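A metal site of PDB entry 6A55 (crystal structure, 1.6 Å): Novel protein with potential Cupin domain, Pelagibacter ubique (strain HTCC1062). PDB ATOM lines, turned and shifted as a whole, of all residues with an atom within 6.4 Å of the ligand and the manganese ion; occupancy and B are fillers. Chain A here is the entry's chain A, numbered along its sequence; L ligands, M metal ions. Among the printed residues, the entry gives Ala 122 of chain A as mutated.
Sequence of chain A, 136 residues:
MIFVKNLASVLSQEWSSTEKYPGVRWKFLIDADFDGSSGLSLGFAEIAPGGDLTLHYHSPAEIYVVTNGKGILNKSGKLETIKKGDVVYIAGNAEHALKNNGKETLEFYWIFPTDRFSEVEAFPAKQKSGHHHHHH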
ATOM      1  N   TYR A  21     -17.544   7.445 -10.418  1.00  0.00           N
ATOM      2  CA  TYR A  21     -16.924   6.131 -10.296  1.00  0.00           C
ATOM      3  C   TYR A  21     -17.386   5.390  -9.037  1.00  0.00           C
ATOM      4  O   TYR A  21     -16.718   5.454  -8.002  1.00  0.00           O
ATOM      5  CB  TYR A  21     -15.396   6.252 -10.247  1.00  0.00           C
ATOM      6  CG  TYR A  21     -14.792   7.014 -11.397  1.00  0.00           C
ATOM      7  CD1 TYR A  21     -15.337   6.957 -12.671  1.00  0.00           C
ATOM      8  CD2 TYR A  21     -13.660   7.806 -11.202  1.00  0.00           C
ATOM      9  CE1 TYR A  21     -14.765   7.667 -13.728  1.00  0.00           C
ATOM     10  CE2 TYR A  21     -13.090   8.526 -12.259  1.00  0.00           C
ATOM     11  CZ  TYR A  21     -13.650   8.444 -13.511  1.00  0.00           C
ATOM     12  OH  TYR A  21     -13.089   9.141 -14.567  1.00  0.00           O
ATOM     13  N   VAL A  24     -15.084   3.094  -6.220  1.00  0.00           N
ATOM     14  CA  VAL A  24     -13.657   3.314  -6.457  1.00  0.00           C
ATOM     15  C   VAL A  24     -13.124   4.354  -5.480  1.00  0.00           C
ATOM     16  O   VAL A  24     -13.792   5.352  -5.212  1.00  0.00           O
ATOM     17  CB  VAL A  24     -13.406   3.799  -7.905  1.00  0.00           C
ATOM     18  CG1 VAL A  24     -11.921   3.889  -8.187  1.00  0.00           C
ATOM     19  CG2 VAL A  24     -14.098   2.892  -8.905  1.00  0.00           C
ATOM     20  N   ARG A  25     -11.930   4.109  -4.945  1.00  0.00           N
ATOM     21  CA  ARG A  25     -11.242   5.129  -4.161  1.00  0.00           C
ATOM     22  C   ARG A  25      -9.749   5.077  -4.428  1.00  0.00           C
ATOM     23  O   ARG A  25      -9.222   4.061  -4.869  1.00  0.00           O
ATOM     24  CB  ARG A  25     -11.525   4.971  -2.656  1.00  0.00           C
ATOM     25  CG  ARG A  25     -11.035   3.677  -2.059  1.00  0.00           C
ATOM     26  CD  ARG A  25     -11.346   3.617  -0.569  1.00  0.00           C
ATOM     27  NE  ARG A  25     -10.701   2.464   0.055  1.00  0.00           N
ATOM     28  CZ  ARG A  25     -10.668   2.236   1.358  1.00  0.00           C
ATOM     29  NH1 ARG A  25     -10.057   1.147   1.823  1.00  0.00           N
ATOM     30  NH2 ARG A  25     -11.238   3.089   2.202  1.00  0.00           N
ATOM     31  N   TRP A  26      -9.060   6.188  -4.174  1.00  0.00           N
ATOM     32  CA  TRP A  26      -7.642   6.236  -4.494  1.00  0.00           C
ATOM     33  C   TRP A  26      -6.836   7.172  -3.617  1.00  0.00           C
ATOM     34  O   TRP A  26      -7.386   8.016  -2.918  1.00  0.00           O
ATOM     35  CB  TRP A  26      -7.444   6.611  -5.969  1.00  0.00           C
ATOM     36  CG  TRP A  26      -8.038   7.925  -6.386  1.00  0.00           C
ATOM     37  CD1 TRP A  26      -7.443   9.162  -6.352  1.00  0.00           C
ATOM     38  CD2 TRP A  26      -9.356   8.137  -6.925  1.00  0.00           C
ATOM     39  NE1 TRP A  26      -8.303  10.113  -6.843  1.00  0.00           N
ATOM     40  CE2 TRP A  26      -9.481   9.524  -7.189  1.00  0.00           C
ATOM     41  CE3 TRP A  26     -10.435   7.299  -7.204  1.00  0.00           C
ATOM     42  CZ2 TRP A  26     -10.655  10.069  -7.722  1.00  0.00           C
ATOM     43  CZ3 TRP A  26     -11.595   7.846  -7.738  1.00  0.00           C
ATOM     44  CH2 TRP A  26     -11.694   9.218  -7.985  1.00  0.00           C
ATOM     45  N   PHE A  28      -2.801   9.320  -3.881  1.00  0.00           N
ATOM     46  CA  PHE A  28      -1.722   9.741  -4.754  1.00  0.00           C
ATOM     47  C   PHE A  28      -0.386   9.464  -4.069  1.00  0.00           C
ATOM     48  O   PHE A  28      -0.115  10.010  -3.008  1.00  0.00           O
ATOM     49  CB  PHE A  28      -1.863  11.229  -5.049  1.00  0.00           C
ATOM     50  CG  PHE A  28      -3.226  11.613  -5.549  1.00  0.00           C
ATOM     51  CD1 PHE A  28      -3.622  11.248  -6.819  1.00  0.00           C
ATOM     52  CD2 PHE A  28      -4.110  12.326  -4.745  1.00  0.00           C
ATOM     53  CE1 PHE A  28      -4.872  11.581  -7.289  1.00  0.00           C
ATOM     54  CE2 PHE A  28      -5.363  12.669  -5.229  1.00  0.00           C
ATOM     55  CZ  PHE A  28      -5.742  12.287  -6.501  1.00  0.00           C
ATOM     56  N   PHE A  44      -2.631   4.904  -6.304  1.00  0.00           N
ATOM     57  CA  PHE A  44      -3.081   3.573  -5.949  1.00  0.00           C
ATOM     58  C   PHE A  44      -4.590   3.586  -5.795  1.00  0.00           C
ATOM     59  O   PHE A  44      -5.126   4.464  -5.103  1.00  0.00           O
ATOM     60  CB  PHE A  44      -2.427   3.099  -4.647  1.00  0.00           C
ATOM     61  CG  PHE A  44      -2.916   1.754  -4.183  1.00  0.00           C
ATOM     62  CD1 PHE A  44      -2.485   0.597  -4.812  1.00  0.00           C
ATOM     63  CD2 PHE A  44      -3.812   1.654  -3.131  1.00  0.00           C
ATOM     64  CE1 PHE A  44      -2.940  -0.647  -4.403  1.00  0.00           C
ATOM     65  CE2 PHE A  44      -4.266   0.410  -2.708  1.00  0.00           C
ATOM     66  CZ  PHE A  44      -3.831  -0.735  -3.344  1.00  0.00           C
ATOM     67  N   ALA A  45      -5.268   2.652  -6.435  1.00  0.00           N
ATOM     68  CA  ALA A  45      -6.730   2.622  -6.423  1.00  0.00           C
ATOM     69  C   ALA A  45      -7.276   1.285  -5.938  1.00  0.00           C
ATOM     70  O   ALA A  45      -6.680   0.231  -6.173  1.00  0.00           O
ATOM     71  CB  ALA A  45      -7.286   2.936  -7.809  1.00  0.00           C
ATOM     72  N   LEU A  53     -14.846   1.739 -12.509  1.00  0.00           N
ATOM     73  CA  LEU A  53     -14.129   2.896 -13.023  1.00  0.00           C
ATOM     74  C   LEU A  53     -14.754   3.124 -14.392  1.00  0.00           C
ATOM     75  O   LEU A  53     -14.323   2.538 -15.384  1.00  0.00           O
ATOM     76  CB  LEU A  53     -12.630   2.623 -13.135  1.00  0.00           C
ATOM     77  CG  LEU A  53     -11.722   3.807 -13.459  1.00  0.00           C
ATOM     78  CD1 LEU A  53     -11.798   4.866 -12.376  1.00  0.00           C
ATOM     79  CD2 LEU A  53     -10.271   3.346 -13.652  1.00  0.00           C
ATOM     80  N   HIS A  56     -14.211   6.064 -19.771  1.00  0.00           N
ATOM     81  CA  HIS A  56     -13.706   7.425 -19.916  1.00  0.00           C
ATOM     82  C   HIS A  56     -12.465   7.438 -20.783  1.00  0.00           C
ATOM     83  O   HIS A  56     -11.966   6.395 -21.187  1.00  0.00           O
ATOM     84  CB  HIS A  56     -13.362   8.019 -18.548  1.00  0.00           C
ATOM     85  CG  HIS A  56     -12.195   7.353 -17.876  1.00  0.00           C
ATOM     86  ND1 HIS A  56     -12.311   6.151 -17.206  1.00  0.00           N
ATOM     87  CD2 HIS A  56     -10.901   7.723 -17.783  1.00  0.00           C
ATOM     88  CE1 HIS A  56     -11.131   5.805 -16.731  1.00  0.00           C
ATOM     89  NE2 HIS A  56     -10.254   6.748 -17.054  1.00  0.00           N
ATOM     90  N   TYR A  57     -11.954   8.635 -21.064  1.00  0.00           N
ATOM     91  CA  TYR A  57     -10.693   8.766 -21.757  1.00  0.00           C
ATOM     92  C   TYR A  57      -9.997  10.040 -21.306  1.00  0.00           C
ATOM     93  O   TYR A  57     -10.595  10.887 -20.644  1.00  0.00           O
ATOM     94  CB  TYR A  57     -10.884   8.791 -23.274  1.00  0.00           C
ATOM     95  CG  TYR A  57     -11.675   9.970 -23.776  1.00  0.00           C
ATOM     96  CD1 TYR A  57     -13.059   9.917 -23.835  1.00  0.00           C
ATOM     97  CD2 TYR A  57     -11.044  11.125 -24.190  1.00  0.00           C
ATOM     98  CE1 TYR A  57     -13.792  11.003 -24.297  1.00  0.00           C
ATOM     99  CE2 TYR A  57     -11.763  12.214 -24.652  1.00  0.00           C
ATOM    100  CZ  TYR A  57     -13.135  12.143 -24.706  1.00  0.00           C
ATOM    101  OH  TYR A  57     -13.873  13.218 -25.161  1.00  0.00           O
ATOM    102  N   HIS A  58      -8.726  10.154 -21.667  1.00  0.00           N
ATOM    103  CA  HIS A  58      -7.972  11.357 -21.380  1.00  0.00           C
ATOM    104  C   HIS A  58      -6.766  11.408 -22.306  1.00  0.00           C
ATOM    105  O   HIS A  58      -6.363  10.393 -22.849  1.00  0.00           O
ATOM    106  CB  HIS A  58      -7.553  11.399 -19.910  1.00  0.00           C
ATOM    107  CG  HIS A  58      -7.311  10.037 -19.321  1.00  0.00           C
ATOM    108  ND1 HIS A  58      -6.446   9.125 -19.896  1.00  0.00           N
ATOM    109  CD2 HIS A  58      -7.809   9.451 -18.217  1.00  0.00           C
ATOM    110  CE1 HIS A  58      -6.433   8.026 -19.163  1.00  0.00           C
ATOM    111  NE2 HIS A  58      -7.256   8.198 -18.136  1.00  0.00           N
ATOM    112  N   GLU A  62      -1.707   5.866 -20.479  1.00  0.00           N
ATOM    113  CA  GLU A  62      -1.770   5.463 -19.095  1.00  0.00           C
ATOM    114  C   GLU A  62      -1.401   3.997 -18.963  1.00  0.00           C
ATOM    115  O   GLU A  62      -1.608   3.222 -19.903  1.00  0.00           O
ATOM    116  CB  GLU A  62      -3.178   5.679 -18.553  1.00  0.00           C
ATOM    117  CG  GLU A  62      -3.323   5.406 -17.065  1.00  0.00           C
ATOM    118  CD  GLU A  62      -4.714   5.668 -16.551  1.00  0.00           C
ATOM    119  OE1 GLU A  62      -5.650   5.725 -17.386  1.00  0.00           O
ATOM    120  OE2 GLU A  62      -4.871   5.816 -15.323  1.00  0.00           O
ATOM    121  N   TYR A  64      -1.907   0.694 -16.138  1.00  0.00           N
ATOM    122  CA  TYR A  64      -2.373   0.116 -14.887  1.00  0.00           C
ATOM    123  C   TYR A  64      -1.455  -1.030 -14.523  1.00  0.00           C
ATOM    124  O   TYR A  64      -1.037  -1.789 -15.392  1.00  0.00           O
ATOM    125  CB  TYR A  64      -3.779  -0.467 -15.013  1.00  0.00           C
ATOM    126  CG  TYR A  64      -4.898   0.502 -15.266  1.00  0.00           C
ATOM    127  CD1 TYR A  64      -4.844   1.803 -14.797  1.00  0.00           C
ATOM    128  CD2 TYR A  64      -6.034   0.103 -15.944  1.00  0.00           C
ATOM    129  CE1 TYR A  64      -5.894   2.692 -15.023  1.00  0.00           C
ATOM    130  CE2 TYR A  64      -7.072   0.964 -16.179  1.00  0.00           C
ATOM    131  CZ  TYR A  64      -7.009   2.258 -15.718  1.00  0.00           C
ATOM    132  OH  TYR A  64      -8.061   3.107 -15.967  1.00  0.00           O
ATOM    133  N   ILE A  90      -2.918   1.813 -21.951  1.00  0.00           N
ATOM    134  CA  ILE A  90      -4.038   2.535 -22.533  1.00  0.00           C
ATOM    135  C   ILE A  90      -3.502   3.695 -23.378  1.00  0.00           C
ATOM    136  O   ILE A  90      -2.919   4.636 -22.829  1.00  0.00           O
ATOM    137  CB  ILE A  90      -4.980   3.077 -21.446  1.00  0.00           C
ATOM    138  CG1 ILE A  90      -5.434   1.938 -20.515  1.00  0.00           C
ATOM    139  CG2 ILE A  90      -6.178   3.776 -22.070  1.00  0.00           C
ATOM    140  CD1 ILE A  90      -5.427   2.299 -19.067  1.00  0.00           C
ATOM    141  N   HIS A  96     -11.767   3.704 -22.021  1.00  0.00           N
ATOM    142  CA  HIS A  96     -11.554   2.517 -21.196  1.00  0.00           C
ATOM    143  C   HIS A  96     -12.330   2.570 -19.894  1.00  0.00           C
ATOM    144  O   HIS A  96     -12.662   3.651 -19.383  1.00  0.00           O
ATOM    145  CB  HIS A  96     -10.072   2.320 -20.899  1.00  0.00           C
ATOM    146  CG  HIS A  96      -9.428   3.502 -20.247  1.00  0.00           C
ATOM    147  ND1 HIS A  96      -9.261   4.713 -20.900  1.00  0.00           N
ATOM    148  CD2 HIS A  96      -8.901   3.670 -19.017  1.00  0.00           C
ATOM    149  CE1 HIS A  96      -8.669   5.569 -20.085  1.00  0.00           C
ATOM    150  NE2 HIS A  96      -8.449   4.958 -18.934  1.00  0.00           N
ATOM    151  N   PHE A 108      -4.934  -1.712  -7.911  1.00  0.00           N
ATOM    152  CA  PHE A 108      -3.947  -1.443  -8.944  1.00  0.00           C
ATOM    153  C   PHE A 108      -3.314  -0.074  -8.761  1.00  0.00           C
ATOM    154  O   PHE A 108      -3.908   0.807  -8.141  1.00  0.00           O
ATOM    155  CB  PHE A 108      -4.589  -1.533 -10.331  1.00  0.00           C
ATOM    156  CG  PHE A 108      -5.733  -0.571 -10.553  1.00  0.00           C
ATOM    157  CD1 PHE A 108      -7.030  -0.924 -10.212  1.00  0.00           C
ATOM    158  CD2 PHE A 108      -5.516   0.685 -11.103  1.00  0.00           C
ATOM    159  CE1 PHE A 108      -8.090  -0.048 -10.410  1.00  0.00           C
ATOM    160  CE2 PHE A 108      -6.576   1.561 -11.300  1.00  0.00           C
ATOM    161  CZ  PHE A 108      -7.856   1.200 -10.947  1.00  0.00           C
ATOM    162  N   TRP A 110      -1.990   3.192 -10.973  1.00  0.00           N
ATOM    163  CA  TRP A 110      -2.002   3.773 -12.315  1.00  0.00           C
ATOM    164  C   TRP A 110      -0.807   4.686 -12.448  1.00  0.00           C
ATOM    165  O   TRP A 110      -0.321   5.247 -11.456  1.00  0.00           O
ATOM    166  CB  TRP A 110      -3.299   4.535 -12.587  1.00  0.00           C
ATOM    167  CG  TRP A 110      -3.330   5.893 -11.980  1.00  0.00           C
ATOM    168  CD1 TRP A 110      -2.815   7.042 -12.504  1.00  0.00           C
ATOM    169  CD2 TRP A 110      -3.903   6.253 -10.720  1.00  0.00           C
ATOM    170  NE1 TRP A 110      -3.040   8.095 -11.649  1.00  0.00           N
ATOM    171  CE2 TRP A 110      -3.710   7.639 -10.553  1.00  0.00           C
ATOM    172  CE3 TRP A 110      -4.573   5.538  -9.719  1.00  0.00           C
ATOM    173  CZ2 TRP A 110      -4.155   8.317  -9.421  1.00  0.00           C
ATOM    174  CZ3 TRP A 110      -5.019   6.216  -8.601  1.00  0.00           C
ATOM    175  CH2 TRP A 110      -4.805   7.597  -8.457  1.00  0.00           C
ATOM    176  N   PHE A 112       0.664   7.921 -15.058  1.00  0.00           N
ATOM    177  CA  PHE A 112       0.544   8.837 -16.193  1.00  0.00           C
ATOM    178  C   PHE A 112       1.902   9.454 -16.480  1.00  0.00           C
ATOM    179  O   PHE A 112       2.726   9.626 -15.569  1.00  0.00           O
ATOM    180  CB  PHE A 112      -0.403   9.991 -15.858  1.00  0.00           C
ATOM    181  CG  PHE A 112      -1.864   9.638 -15.914  1.00  0.00           C
ATOM    182  CD1 PHE A 112      -2.469   9.299 -17.115  1.00  0.00           C
ATOM    183  CD2 PHE A 112      -2.644   9.719 -14.767  1.00  0.00           C
ATOM    184  CE1 PHE A 112      -3.824   8.997 -17.165  1.00  0.00           C
ATOM    185  CE2 PHE A 112      -3.991   9.418 -14.810  1.00  0.00           C
ATOM    186  CZ  PHE A 112      -4.593   9.060 -16.012  1.00  0.00           C
ATOM    187  N   PHE A 117      -1.717  14.222 -11.149  1.00  0.00           N
ATOM    188  CA  PHE A 117      -3.005  13.688 -11.561  1.00  0.00           C
ATOM    189  C   PHE A 117      -3.913  14.812 -12.027  1.00  0.00           C
ATOM    190  O   PHE A 117      -4.701  14.627 -12.963  1.00  0.00           O
ATOM    191  CB  PHE A 117      -3.639  12.939 -10.380  1.00  0.00           C
ATOM    192  CG  PHE A 117      -4.974  12.327 -10.677  1.00  0.00           C
ATOM    193  CD1 PHE A 117      -5.066  11.144 -11.387  1.00  0.00           C
ATOM    194  CD2 PHE A 117      -6.145  12.920 -10.200  1.00  0.00           C
ATOM    195  CE1 PHE A 117      -6.304  10.570 -11.635  1.00  0.00           C
ATOM    196  CE2 PHE A 117      -7.369  12.348 -10.449  1.00  0.00           C
ATOM    197  CZ  PHE A 117      -7.456  11.176 -11.166  1.00  0.00           C
ATOM    198  N   VAL A 120      -4.455  15.749 -15.630  1.00  0.00           N
ATOM    199  CA  VAL A 120      -5.126  14.819 -16.512  1.00  0.00           C
ATOM    200  C   VAL A 120      -6.635  14.989 -16.417  1.00  0.00           C
ATOM    201  O   VAL A 120      -7.234  14.694 -15.385  1.00  0.00           O
ATOM    202  CB  VAL A 120      -4.737  13.368 -16.189  1.00  0.00           C
ATOM    203  CG1 VAL A 120      -5.342  12.417 -17.206  1.00  0.00           C
ATOM    204  CG2 VAL A 120      -3.217  13.225 -16.178  1.00  0.00           C
ATOM    205  N   ALA A 122     -10.211  13.919 -17.250  1.00  0.00           N
ATOM    206  CA  ALA A 122     -10.949  12.727 -17.667  1.00  0.00           C
ATOM    207  C   ALA A 122     -12.304  13.107 -18.253  1.00  0.00           C
ATOM    208  O   ALA A 122     -13.082  13.829 -17.622  1.00  0.00           O
ATOM    209  CB  ALA A 122     -11.116  11.774 -16.500  1.00  0.00           C
HETATM  210  S1  LIG L   1      -8.670   7.294 -10.728  1.00  0.00           S
HETATM  211  C1  LIG L   1      -7.979   6.404 -14.575  1.00  0.00           C
HETATM  212  O1  LIG L   1      -8.222   7.481 -15.174  1.00  0.00           O
HETATM  213  C2  LIG L   1      -8.080   6.313 -13.077  1.00  0.00           C
HETATM  214  O2  LIG L   1      -7.654   5.370 -15.226  1.00  0.00           O
HETATM  215  C3  LIG L   1      -8.687   7.549 -12.472  1.00  0.00           C
HETATM  216  C4  LIG L   1      -8.248   5.748 -10.240  1.00  0.00           C
HETATM  217  C5  LIG L   1      -7.960   8.363  -9.652  1.00  0.00           C
HETATM  218 MN    MN M   1      -7.896   6.212 -17.134  1.00  0.00          MN
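Residues that only touch the ligand: Trp 26, Phe 117, Trp 110, Leu 53 and Ala 45. Ten residues have an atom within 4 Å of the ligand: Trp 26, Ala 45, Leu 53, His 56, His 58, Glu 62, Tyr 64, His 96, Trp 110 and Phe 117. The nearest printed residue that does not touch the ligand is Phe 112 (4.05 Å).
O2 of the ligand sits close to OH of Tyr 64, 2.4 Å away.
The manganese ion is bound by O2 of the ligand, at 2.1 Å. The manganese ion is bound by NE2 of His 96 (2.3 Å). OE1 of Glu 62 binds the manganese ion. NE2 of His 58 is bound to the manganese ion, 2.3 Å away. The manganese ion is bound by O1 of the ligand (2.4 Å). The manganese ion is bound by NE2 of His 56, 2.4 Å away. The manganese ion has six donor atoms within binding distance.
O of Glu 62 is in hydrogen-bond range of N of Ile 90, at 2.8 Å. The backbone NH (N) of Ala 45 lies within hydrogen-bond range of the backbone carbonyl oxygen (O) of Phe 108.
Tyr 64 touches the manganese ion. The nearest printed residue that does not touch the manganese ion is Phe 112 (4.5 Å).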
